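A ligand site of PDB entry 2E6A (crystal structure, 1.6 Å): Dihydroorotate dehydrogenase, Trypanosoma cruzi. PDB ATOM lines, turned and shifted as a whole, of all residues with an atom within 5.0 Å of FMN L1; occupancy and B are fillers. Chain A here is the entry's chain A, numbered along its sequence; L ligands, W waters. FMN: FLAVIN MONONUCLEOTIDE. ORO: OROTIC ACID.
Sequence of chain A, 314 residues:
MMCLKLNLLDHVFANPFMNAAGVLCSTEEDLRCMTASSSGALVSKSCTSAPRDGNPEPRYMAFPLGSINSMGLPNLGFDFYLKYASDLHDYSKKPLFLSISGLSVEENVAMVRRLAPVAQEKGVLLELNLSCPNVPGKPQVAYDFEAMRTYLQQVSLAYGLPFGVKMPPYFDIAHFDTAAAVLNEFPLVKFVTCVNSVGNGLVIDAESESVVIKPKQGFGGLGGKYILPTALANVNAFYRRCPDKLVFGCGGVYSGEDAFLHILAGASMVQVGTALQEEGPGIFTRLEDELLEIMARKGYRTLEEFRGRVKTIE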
ATOM      1  N   ALA A  20     -16.138  -2.919 -25.113  1.00  0.00           N
ATOM      2  CA  ALA A  20     -17.153  -3.934 -25.375  1.00  0.00           C
ATOM      3  C   ALA A  20     -18.026  -4.087 -24.134  1.00  0.00           C
ATOM      4  O   ALA A  20     -17.526  -3.941 -23.019  1.00  0.00           O
ATOM      5  CB  ALA A  20     -16.482  -5.258 -25.748  1.00  0.00           C
ATOM      6  N   ALA A  21     -19.330  -4.344 -24.317  1.00  0.00           N
ATOM      7  CA  ALA A  21     -20.209  -4.540 -23.165  1.00  0.00           C
ATOM      8  C   ALA A  21     -19.661  -5.601 -22.226  1.00  0.00           C
ATOM      9  O   ALA A  21     -19.126  -6.611 -22.670  1.00  0.00           O
ATOM     10  CB  ALA A  21     -21.624  -4.884 -23.598  1.00  0.00           C
ATOM     11  N   GLY A  22     -19.768  -5.348 -20.929  1.00  0.00           N
ATOM     12  CA  GLY A  22     -19.331  -6.328 -19.929  1.00  0.00           C
ATOM     13  C   GLY A  22     -17.931  -6.080 -19.418  1.00  0.00           C
ATOM     14  O   GLY A  22     -17.592  -6.541 -18.316  1.00  0.00           O
ATOM     15  N   VAL A  23     -17.128  -5.338 -20.168  1.00  0.00           N
ATOM     16  CA  VAL A  23     -15.743  -5.058 -19.776  1.00  0.00           C
ATOM     17  C   VAL A  23     -15.639  -3.626 -19.222  1.00  0.00           C
ATOM     18  O   VAL A  23     -15.992  -2.670 -19.916  1.00  0.00           O
ATOM     19  CB  VAL A  23     -14.763  -5.267 -20.958  1.00  0.00           C
ATOM     20  CG1 VAL A  23     -13.343  -4.952 -20.511  1.00  0.00           C
ATOM     21  CG2 VAL A  23     -14.858  -6.722 -21.477  1.00  0.00           C
ATOM     22  N   LYS A  45     -22.591  -2.606 -18.580  1.00  0.00           N
ATOM     23  CA  LYS A  45     -22.741  -4.065 -18.463  1.00  0.00           C
ATOM     24  C   LYS A  45     -24.158  -4.494 -18.847  1.00  0.00           C
ATOM     25  O   LYS A  45     -25.130  -3.873 -18.403  1.00  0.00           O
ATOM     26  CB  LYS A  45     -22.474  -4.457 -16.993  1.00  0.00           C
ATOM     27  CG  LYS A  45     -22.846  -5.913 -16.635  1.00  0.00           C
ATOM     28  CD  LYS A  45     -21.924  -6.917 -17.328  1.00  0.00           C
ATOM     29  CE  LYS A  45     -22.462  -8.347 -17.223  1.00  0.00           C
ATOM     30  NZ  LYS A  45     -21.567  -9.269 -18.031  1.00  0.00           N
ATOM     31  N   SER A  46     -24.296  -5.572 -19.618  1.00  0.00           N
ATOM     32  CA  SER A  46     -25.649  -6.071 -19.930  1.00  0.00           C
ATOM     33  C   SER A  46     -26.377  -6.374 -18.633  1.00  0.00           C
ATOM     34  O   SER A  46     -25.869  -7.125 -17.775  1.00  0.00           O
ATOM     35  CB  SER A  46     -25.608  -7.342 -20.778  1.00  0.00           C
ATOM     36  OG  SER A  46     -25.187  -7.023 -22.067  1.00  0.00           O
ATOM     37  N   TYR A  60     -13.557 -16.050 -15.306  1.00  0.00           N
ATOM     38  CA  TYR A  60     -12.852 -15.425 -16.403  1.00  0.00           C
ATOM     39  C   TYR A  60     -11.390 -15.813 -16.338  1.00  0.00           C
ATOM     40  O   TYR A  60     -10.786 -15.796 -15.250  1.00  0.00           O
ATOM     41  CB  TYR A  60     -12.961 -13.912 -16.302  1.00  0.00           C
ATOM     42  CG  TYR A  60     -12.054 -13.172 -17.277  1.00  0.00           C
ATOM     43  CD1 TYR A  60     -10.784 -12.730 -16.895  1.00  0.00           C
ATOM     44  CD2 TYR A  60     -12.464 -12.928 -18.587  1.00  0.00           C
ATOM     45  CE1 TYR A  60      -9.936 -12.054 -17.813  1.00  0.00           C
ATOM     46  CE2 TYR A  60     -11.625 -12.254 -19.508  1.00  0.00           C
ATOM     47  CZ  TYR A  60     -10.377 -11.824 -19.108  1.00  0.00           C
ATOM     48  OH  TYR A  60      -9.552 -11.159 -20.000  1.00  0.00           O
ATOM     49  N   SER A  67      -9.275 -14.797 -24.295  1.00  0.00           N
ATOM     50  CA  SER A  67      -9.901 -15.073 -23.012  1.00  0.00           C
ATOM     51  C   SER A  67     -11.052 -16.053 -23.140  1.00  0.00           C
ATOM     52  O   SER A  67     -11.580 -16.283 -24.232  1.00  0.00           O
ATOM     53  CB  SER A  67     -10.425 -13.771 -22.400  1.00  0.00           C
ATOM     54  OG  SER A  67     -11.485 -13.275 -23.183  1.00  0.00           O
ATOM     55  N   ASN A  69     -14.746 -16.783 -20.825  1.00  0.00           N
ATOM     56  CA  ASN A  69     -15.539 -16.271 -19.707  1.00  0.00           C
ATOM     57  C   ASN A  69     -16.880 -16.938 -19.619  1.00  0.00           C
ATOM     58  O   ASN A  69     -17.486 -17.254 -20.636  1.00  0.00           O
ATOM     59  CB  ASN A  69     -15.716 -14.733 -19.776  1.00  0.00           C
ATOM     60  CG  ASN A  69     -16.948 -14.293 -20.579  1.00  0.00           C
ATOM     61  OD1 ASN A  69     -18.077 -14.257 -20.077  1.00  0.00           O
ATOM     62  ND2 ASN A  69     -16.725 -13.945 -21.840  1.00  0.00           N
ATOM     63  N   MET A  71     -19.271 -15.378 -17.184  1.00  0.00           N
ATOM     64  CA  MET A  71     -19.614 -14.494 -16.061  1.00  0.00           C
ATOM     65  C   MET A  71     -21.026 -14.773 -15.525  1.00  0.00           C
ATOM     66  O   MET A  71     -21.223 -14.814 -14.310  1.00  0.00           O
ATOM     67  CB  MET A  71     -19.469 -13.023 -16.447  1.00  0.00           C
ATOM     68  CG  MET A  71     -18.160 -12.661 -17.136  1.00  0.00           C
ATOM     69  SD  MET A  71     -16.722 -12.958 -16.100  1.00  0.00           S
ATOM     70  CE  MET A  71     -16.988 -11.758 -14.799  1.00  0.00           C
ATOM     71  N   LEU A  73     -23.878 -12.947 -16.455  1.00  0.00           N
ATOM     72  CA  LEU A  73     -24.575 -11.648 -16.300  1.00  0.00           C
ATOM     73  C   LEU A  73     -24.599 -11.133 -14.858  1.00  0.00           C
ATOM     74  O   LEU A  73     -25.652 -10.714 -14.360  1.00  0.00           O
ATOM     75  CB  LEU A  73     -25.990 -11.705 -16.895  1.00  0.00           C
ATOM     76  CG  LEU A  73     -26.084 -11.903 -18.403  1.00  0.00           C
ATOM     77  CD1 LEU A  73     -27.533 -12.156 -18.811  1.00  0.00           C
ATOM     78  CD2 LEU A  73     -25.528 -10.691 -19.139  1.00  0.00           C
ATOM     79  N   SER A  99     -26.690  -1.471 -22.294  1.00  0.00           N
ATOM     80  CA  SER A  99     -26.944  -2.813 -22.816  1.00  0.00           C
ATOM     81  C   SER A  99     -27.931  -3.557 -21.909  1.00  0.00           C
ATOM     82  O   SER A  99     -27.785  -3.554 -20.688  1.00  0.00           O
ATOM     83  CB  SER A  99     -25.634  -3.602 -22.927  1.00  0.00           C
ATOM     84  OG  SER A  99     -25.901  -4.957 -23.307  1.00  0.00           O
ATOM     85  N   GLU A 127     -28.561  -0.890 -26.527  1.00  0.00           N
ATOM     86  CA  GLU A 127     -28.004  -2.075 -27.226  1.00  0.00           C
ATOM     87  C   GLU A 127     -28.698  -3.309 -26.619  1.00  0.00           C
ATOM     88  O   GLU A 127     -28.554  -3.567 -25.423  1.00  0.00           O
ATOM     89  CB  GLU A 127     -26.453  -2.150 -27.102  1.00  0.00           C
ATOM     90  CG  GLU A 127     -25.743  -3.323 -27.914  1.00  0.00           C
ATOM     91  CD  GLU A 127     -24.182  -3.353 -27.844  1.00  0.00           C
ATOM     92  OE1 GLU A 127     -23.634  -3.905 -26.864  1.00  0.00           O
ATOM     93  OE2 GLU A 127     -23.477  -2.861 -28.784  1.00  0.00           O
ATOM     94  N   ASN A 129     -29.032  -7.089 -26.120  1.00  0.00           N
ATOM     95  CA  ASN A 129     -28.129  -8.247 -26.196  1.00  0.00           C
ATOM     96  C   ASN A 129     -28.901  -9.541 -26.501  1.00  0.00           C
ATOM     97  O   ASN A 129     -29.603 -10.065 -25.650  1.00  0.00           O
ATOM     98  CB  ASN A 129     -27.354  -8.360 -24.874  1.00  0.00           C
ATOM     99  CG  ASN A 129     -26.322  -9.453 -24.878  1.00  0.00           C
ATOM    100  OD1 ASN A 129     -26.203 -10.202 -25.845  1.00  0.00           O
ATOM    101  ND2 ASN A 129     -25.548  -9.548 -23.795  1.00  0.00           N
ATOM    102  N   LYS A 166     -26.802  -6.597 -30.183  1.00  0.00           N
ATOM    103  CA  LYS A 166     -25.529  -7.311 -30.072  1.00  0.00           C
ATOM    104  C   LYS A 166     -25.738  -8.743 -30.566  1.00  0.00           C
ATOM    105  O   LYS A 166     -26.532  -9.485 -29.978  1.00  0.00           O
ATOM    106  CB  LYS A 166     -25.048  -7.293 -28.599  1.00  0.00           C
ATOM    107  CG  LYS A 166     -23.713  -8.019 -28.362  1.00  0.00           C
ATOM    108  CD  LYS A 166     -22.544  -7.213 -28.920  1.00  0.00           C
ATOM    109  CE  LYS A 166     -21.196  -7.712 -28.395  1.00  0.00           C
ATOM    110  NZ  LYS A 166     -20.962  -7.427 -26.959  1.00  0.00           N
ATOM    111  N   VAL A 195     -18.983  -8.897 -32.979  1.00  0.00           N
ATOM    112  CA  VAL A 195     -19.761 -10.004 -32.453  1.00  0.00           C
ATOM    113  C   VAL A 195     -19.590 -10.088 -30.931  1.00  0.00           C
ATOM    114  O   VAL A 195     -18.626  -9.552 -30.355  1.00  0.00           O
ATOM    115  CB  VAL A 195     -19.288 -11.366 -33.059  1.00  0.00           C
ATOM    116  CG1 VAL A 195     -19.637 -11.446 -34.560  1.00  0.00           C
ATOM    117  CG2 VAL A 195     -17.790 -11.581 -32.829  1.00  0.00           C
ATOM    118  N   ASN A 196     -20.537 -10.781 -30.298  1.00  0.00           N
ATOM    119  CA  ASN A 196     -20.367 -11.300 -28.948  1.00  0.00           C
ATOM    120  C   ASN A 196     -19.299 -12.417 -28.952  1.00  0.00           C
ATOM    121  O   ASN A 196     -18.767 -12.784 -30.006  1.00  0.00           O
ATOM    122  CB  ASN A 196     -21.710 -11.836 -28.433  1.00  0.00           C
ATOM    123  CG  ASN A 196     -21.867 -11.676 -26.932  1.00  0.00           C
ATOM    124  OD1 ASN A 196     -20.975 -12.018 -26.148  1.00  0.00           O
ATOM    125  ND2 ASN A 196     -23.019 -11.155 -26.526  1.00  0.00           N
ATOM    126  N   SER A 197     -18.993 -12.944 -27.768  1.00  0.00           N
ATOM    127  CA  SER A 197     -17.974 -13.982 -27.657  1.00  0.00           C
ATOM    128  C   SER A 197     -18.377 -15.223 -28.436  1.00  0.00           C
ATOM    129  O   SER A 197     -19.587 -15.499 -28.659  1.00  0.00           O
ATOM    130  CB  SER A 197     -17.720 -14.315 -26.186  1.00  0.00           C
ATOM    131  OG  SER A 197     -18.907 -14.779 -25.584  1.00  0.00           O
ATOM    132  N   LEU A 222     -15.467 -17.333 -25.937  1.00  0.00           N
ATOM    133  CA  LEU A 222     -14.098 -16.955 -26.297  1.00  0.00           C
ATOM    134  C   LEU A 222     -14.013 -15.539 -26.854  1.00  0.00           C
ATOM    135  O   LEU A 222     -14.845 -15.118 -27.664  1.00  0.00           O
ATOM    136  CB  LEU A 222     -13.532 -17.931 -27.343  1.00  0.00           C
ATOM    137  CG  LEU A 222     -13.573 -19.419 -26.996  1.00  0.00           C
ATOM    138  CD1 LEU A 222     -13.149 -20.251 -28.219  1.00  0.00           C
ATOM    139  CD2 LEU A 222     -12.690 -19.735 -25.796  1.00  0.00           C
ATOM    140  N   GLY A 223     -12.974 -14.826 -26.434  1.00  0.00           N
ATOM    141  CA  GLY A 223     -12.665 -13.509 -26.965  1.00  0.00           C
ATOM    142  C   GLY A 223     -11.179 -13.398 -27.263  1.00  0.00           C
ATOM    143  O   GLY A 223     -10.396 -14.280 -26.899  1.00  0.00           O
ATOM    144  N   GLY A 224     -10.781 -12.306 -27.907  1.00  0.00           N
ATOM    145  CA  GLY A 224      -9.365 -12.024 -28.135  1.00  0.00           C
ATOM    146  C   GLY A 224      -8.841 -12.476 -29.489  1.00  0.00           C
ATOM    147  O   GLY A 224      -9.580 -12.544 -30.467  1.00  0.00           O
ATOM    148  N   ILE A 227     -10.499 -14.881 -32.093  1.00  0.00           N
ATOM    149  CA  ILE A 227     -11.767 -14.625 -32.772  1.00  0.00           C
ATOM    150  C   ILE A 227     -11.734 -13.538 -33.850  1.00  0.00           C
ATOM    151  O   ILE A 227     -12.761 -13.258 -34.450  1.00  0.00           O
ATOM    152  CB  ILE A 227     -12.956 -14.389 -31.780  1.00  0.00           C
ATOM    153  CG1 ILE A 227     -12.987 -12.953 -31.234  1.00  0.00           C
ATOM    154  CG2 ILE A 227     -12.951 -15.444 -30.666  1.00  0.00           C
ATOM    155  CD1 ILE A 227     -14.324 -12.615 -30.570  1.00  0.00           C
ATOM    156  N   CYS A 250     -16.720  -5.742 -33.086  1.00  0.00           N
ATOM    157  CA  CYS A 250     -16.214  -6.185 -31.787  1.00  0.00           C
ATOM    158  C   CYS A 250     -15.599  -7.555 -31.973  1.00  0.00           C
ATOM    159  O   CYS A 250     -16.226  -8.451 -32.556  1.00  0.00           O
ATOM    160  CB  CYS A 250     -17.374  -6.249 -30.779  1.00  0.00           C
ATOM    161  SG  CYS A 250     -16.812  -6.556 -29.092  1.00  0.00           S
ATOM    162  N   GLY A 251     -14.382  -7.735 -31.497  1.00  0.00           N
ATOM    163  CA  GLY A 251     -13.771  -9.059 -31.493  1.00  0.00           C
ATOM    164  C   GLY A 251     -12.337  -8.992 -31.962  1.00  0.00           C
ATOM    165  O   GLY A 251     -12.044  -8.603 -33.090  1.00  0.00           O
ATOM    166  N   GLY A 252     -11.429  -9.323 -31.053  1.00  0.00           N
ATOM    167  CA  GLY A 252     -10.021  -9.473 -31.413  1.00  0.00           C
ATOM    168  C   GLY A 252      -9.243  -8.198 -31.627  1.00  0.00           C
ATOM    169  O   GLY A 252      -8.155  -8.254 -32.217  1.00  0.00           O
ATOM    170  N   VAL A 253      -9.759  -7.057 -31.152  1.00  0.00           N
ATOM    171  CA  VAL A 253      -9.039  -5.788 -31.326  1.00  0.00           C
ATOM    172  C   VAL A 253      -7.989  -5.565 -30.239  1.00  0.00           C
ATOM    173  O   VAL A 253      -8.331  -5.381 -29.055  1.00  0.00           O
ATOM    174  CB  VAL A 253      -9.997  -4.556 -31.372  1.00  0.00           C
ATOM    175  CG1 VAL A 253      -9.177  -3.279 -31.476  1.00  0.00           C
ATOM    176  CG2 VAL A 253     -10.975  -4.662 -32.529  1.00  0.00           C
ATOM    177  N   GLN A 271     -15.283  -1.842 -30.885  1.00  0.00           N
ATOM    178  CA  GLN A 271     -15.353  -2.128 -29.454  1.00  0.00           C
ATOM    179  C   GLN A 271     -14.197  -3.005 -29.033  1.00  0.00           C
ATOM    180  O   GLN A 271     -13.701  -3.824 -29.823  1.00  0.00           O
ATOM    181  CB  GLN A 271     -16.658  -2.803 -29.102  1.00  0.00           C
ATOM    182  CG  GLN A 271     -17.899  -2.053 -29.589  1.00  0.00           C
ATOM    183  CD  GLN A 271     -19.191  -2.674 -29.085  1.00  0.00           C
ATOM    184  OE1 GLN A 271     -19.222  -3.832 -28.667  1.00  0.00           O
ATOM    185  NE2 GLN A 271     -20.270  -1.905 -29.130  1.00  0.00           N
ATOM    186  N   VAL A 272     -13.777  -2.845 -27.783  1.00  0.00           N
ATOM    187  CA  VAL A 272     -12.577  -3.508 -27.282  1.00  0.00           C
ATOM    188  C   VAL A 272     -12.926  -4.223 -25.989  1.00  0.00           C
ATOM    189  O   VAL A 272     -13.324  -3.586 -25.017  1.00  0.00           O
ATOM    190  CB  VAL A 272     -11.464  -2.456 -27.035  1.00  0.00           C
ATOM    191  CG1 VAL A 272     -10.195  -3.134 -26.662  1.00  0.00           C
ATOM    192  CG2 VAL A 272     -11.260  -1.569 -28.304  1.00  0.00           C
ATOM    193  N   GLY A 273     -12.798  -5.556 -26.002  1.00  0.00           N
ATOM    194  CA  GLY A 273     -13.172  -6.369 -24.858  1.00  0.00           C
ATOM    195  C   GLY A 273     -11.961  -6.919 -24.151  1.00  0.00           C
ATOM    196  O   GLY A 273     -11.413  -6.262 -23.263  1.00  0.00           O
ATOM    197  N   THR A 274     -11.553  -8.128 -24.529  1.00  0.00           N
ATOM    198  CA  THR A 274     -10.408  -8.826 -23.913  1.00  0.00           C
ATOM    199  C   THR A 274      -9.174  -7.927 -23.749  1.00  0.00           C
ATOM    200  O   THR A 274      -8.564  -7.930 -22.668  1.00  0.00           O
ATOM    201  CB  THR A 274     -10.041 -10.129 -24.691  1.00  0.00           C
ATOM    202  OG1 THR A 274     -11.160 -11.009 -24.659  1.00  0.00           O
ATOM    203  CG2 THR A 274      -8.824 -10.842 -24.058  1.00  0.00           C
ATOM    204  N   ALA A 275      -8.788  -7.212 -24.798  1.00  0.00           N
ATOM    205  CA  ALA A 275      -7.573  -6.391 -24.722  1.00  0.00           C
ATOM    206  C   ALA A 275      -7.699  -5.292 -23.669  1.00  0.00           C
ATOM    207  O   ALA A 275      -6.726  -4.918 -23.013  1.00  0.00           O
ATOM    208  CB  ALA A 275      -7.249  -5.801 -26.069  1.00  0.00           C
HETATM  209  N1  FMN L   1     -21.046  -8.857 -24.154  1.00  0.00           N
HETATM  210  C2  FMN L   1     -22.292  -8.351 -23.950  1.00  0.00           C
HETATM  211  O2  FMN L   1     -23.002  -8.056 -24.937  1.00  0.00           O
HETATM  212  N3  FMN L   1     -22.738  -8.152 -22.667  1.00  0.00           N
HETATM  213  C4  FMN L   1     -21.978  -8.452 -21.555  1.00  0.00           C
HETATM  214  O4  FMN L   1     -22.379  -8.091 -20.423  1.00  0.00           O
HETATM  215  C4A FMN L   1     -20.697  -8.963 -21.772  1.00  0.00           C
HETATM  216  N5  FMN L   1     -19.864  -9.276 -20.705  1.00  0.00           N
HETATM  217  C5A FMN L   1     -18.578  -9.739 -20.946  1.00  0.00           C
HETATM  218  C6  FMN L   1     -17.764 -10.031 -19.855  1.00  0.00           C
HETATM  219  C7  FMN L   1     -16.471 -10.500 -20.074  1.00  0.00           C
HETATM  220  C7M FMN L   1     -15.523 -10.459 -18.907  1.00  0.00           C
HETATM  221  C8  FMN L   1     -15.999 -10.698 -21.382  1.00  0.00           C
HETATM  222  C8M FMN L   1     -14.519 -10.780 -21.652  1.00  0.00           C
HETATM  223  C9  FMN L   1     -16.832 -10.428 -22.465  1.00  0.00           C
HETATM  224  C9A FMN L   1     -18.120  -9.928 -22.249  1.00  0.00           C
HETATM  225  N10 FMN L   1     -18.964  -9.677 -23.301  1.00  0.00           N
HETATM  226  C10 FMN L   1     -20.235  -9.163 -23.082  1.00  0.00           C
HETATM  227  C1' FMN L   1     -18.579 -10.009 -24.716  1.00  0.00           C
HETATM  228  C2' FMN L   1     -17.783  -8.804 -25.228  1.00  0.00           C
HETATM  229  O2' FMN L   1     -18.621  -7.660 -25.261  1.00  0.00           O
HETATM  230  C3' FMN L   1     -17.253  -9.037 -26.644  1.00  0.00           C
HETATM  231  O3' FMN L   1     -18.357  -9.179 -27.525  1.00  0.00           O
HETATM  232  C4' FMN L   1     -16.351 -10.278 -26.732  1.00  0.00           C
HETATM  233  O4' FMN L   1     -15.522 -10.404 -25.572  1.00  0.00           O
HETATM  234  C5' FMN L   1     -15.447 -10.274 -27.971  1.00  0.00           C
HETATM  235  O5' FMN L   1     -14.617  -9.132 -28.028  1.00  0.00           O
HETATM  236  P   FMN L   1     -13.041  -9.251 -27.658  1.00  0.00           P
HETATM  237  O1P FMN L   1     -12.419 -10.206 -28.634  1.00  0.00           O
HETATM  238  O2P FMN L   1     -12.476  -7.840 -27.715  1.00  0.00           O
HETATM  239  O3P FMN L   1     -12.971  -9.781 -26.256  1.00  0.00           O
HETATM  240  N1  ORO L   2     -20.341 -12.969 -21.375  1.00  0.00           N
HETATM  241  C2  ORO L   2     -20.227 -12.826 -22.710  1.00  0.00           C
HETATM  242  O2  ORO L   2     -19.184 -13.209 -23.307  1.00  0.00           O
HETATM  243  N3  ORO L   2     -21.239 -12.272 -23.427  1.00  0.00           N
HETATM  244  C4  ORO L   2     -22.379 -11.876 -22.831  1.00  0.00           C
HETATM  245  O4  ORO L   2     -23.288 -11.391 -23.520  1.00  0.00           O
HETATM  246  C5  ORO L   2     -22.552 -12.033 -21.445  1.00  0.00           C
HETATM  247  C6  ORO L   2     -21.472 -12.555 -20.737  1.00  0.00           C
HETATM  248  C7  ORO L   2     -21.617 -12.842 -19.291  1.00  0.00           C
HETATM  249  O71 ORO L   2     -22.118 -12.039 -18.460  1.00  0.00           O
HETATM  250  O72 ORO L   2     -21.287 -14.015 -19.012  1.00  0.00           O
HETATM  251  O   HOH W   1      -9.818  -7.382 -27.447  1.00  0.00           O
HETATM  252  O   HOH W   2     -24.721  -5.832 -25.478  1.00  0.00           O
HETATM  253  O   HOH W   3     -12.476  -6.348 -29.970  1.00  0.00           O
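O3' of FMN L1 lies within hydrogen-bond range of O of Val 195 (2.9 Å). The side-chain amide oxygen (OD1) of Asn 69 lies within hydrogen-bond range of a nitrogen (N1) of ORO L2, at 2.9 Å. NZ of Lys 166 is in hydrogen-bond range of O2' of FMN L1 (2.9 Å). The side-chain amide nitrogen (ND2) of Asn 129 lies within hydrogen-bond range of an oxygen (O4) of ORO L2 (2.9 Å). O3' of FMN L1 sits at hydrogen-bond distance from SG of Cys 250 (3.4 Å). The side-chain hydroxyl (OG) of Ser 197 is in hydrogen-bond range of an oxygen (O2) of ORO L2 (2.8 Å). The backbone NH of Ser 46 is in hydrogen-bond range of an oxygen (O4) of FMN L1, 3.3 Å away. An oxygen (O72) of ORO L2 sits at hydrogen-bond distance from the backbone NH of Met 71, 3.0 Å away. A nitrogen (N3) of ORO L2 lies within hydrogen-bond range of the side-chain amide oxygen of Asn 196 (2.7 Å). The backbone carbonyl oxygen of Ala 21 sits close to an oxygen (O2') of FMN L1, at 2.8 Å. N3 of FMN L1 is in hydrogen-bond range of OG of Ser 46 (2.8 Å). N of Leu 73 sits at hydrogen-bond distance from O71 of ORO L2, 2.8 Å away. The backbone NH (N) of Gly 273 lies within hydrogen-bond range of an oxygen (O2P) of FMN L1, at 2.9 Å. The side-chain amino group of Lys 45 sits at hydrogen-bond distance from an oxygen (O4) of FMN L1 (2.8 Å). An oxygen (O71) of ORO L2 lies within salt-bridge range of the side-chain amino group (NZ) of Lys 45 (2.9 Å). The side-chain amide nitrogen (ND2) of Asn 129 is in hydrogen-bond range of an oxygen (O2) of FMN L1 (3.2 Å). N of Thr 274 sits at hydrogen-bond distance from O3P of FMN L1 (2.8 Å). O1P of FMN L1 lies within hydrogen-bond range of N of Gly 252, 2.8 Å away. ND2 of Asn 196 lies within hydrogen-bond range of O2 of FMN L1, 3.5 Å away. OG1 of Thr 274 is in hydrogen-bond range of O3P of FMN L1, 2.7 Å away. N of Gly 224 lies within hydrogen-bond range of O1P of FMN L1, 2.8 Å away.
Merely in contact with FMN L1: Ala 20 (3.3 Å), Gly 22 (3.1 Å), Tyr 60 (3.9 Å), Asn 69 (3.4 Å), Met 71 (3.8 Å), Ser 197 (3.8 Å), Gly 223 (3.7 Å), Ile 227 (3.6 Å) and Gly 251 (3.4 Å). Hydrophobic or aromatic side chains that line FMN L1: Ala 20, Ala 21, Tyr 60, Met 71 and Ile 227. 21 residues have an atom within 4 Å of FMN L1: Ala 20, Ala 21, Gly 22, Lys 45, Ser 46, Tyr 60, Asn 69, Met 71, Asn 129, Lys 166, Val 195, Asn 196, Ser 197, Gly 223, Gly 224, Ile 227, Cys 250, Gly 251, Gly 252, Gly 273 and Thr 274. Along chain A the residues within 4 Å of FMN L1 span positions 20 to 274.
N3 of FMN L1 sits close to O4 of ORO L2, at 3.4 Å.
Water W1 lies within hydrogen-bond range of an oxygen (O2P) of FMN L1, the backbone NH (N) of Ala 275, the backbone carbonyl oxygen (O) of Val 253 and the backbone NH (N) of Thr 274. Water W2 lies within hydrogen-bond range of the side-chain carboxylate of Glu 127, the side-chain hydroxyl of Ser 99 and an oxygen (O2) of FMN L1.
O of Val 272 is in hydrogen-bond range of N of Ala 20 (2.9 Å). ND2 of Asn 129 lies within hydrogen-bond range of OG of Ser 46. The backbone NH of Val 195 sits at hydrogen-bond distance from the backbone carbonyl oxygen of Cys 250 (2.8 Å). OE1 of Gln 271 is in hydrogen-bond range of SG of Cys 250 (3.7 Å). OG1 of Thr 274 lies within hydrogen-bond range of OG of Ser 67. OG of Ser 46 sits at hydrogen-bond distance from OG of Ser 99. The side-chain amide oxygen of Asn 129 lies within hydrogen-bond range of the side-chain amide nitrogen of Asn 196 (3.4 Å). The side-chain amide oxygen (OD1) of Asn 69 lies within hydrogen-bond range of the backbone NH (N) of Met 71 (3.3 Å).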
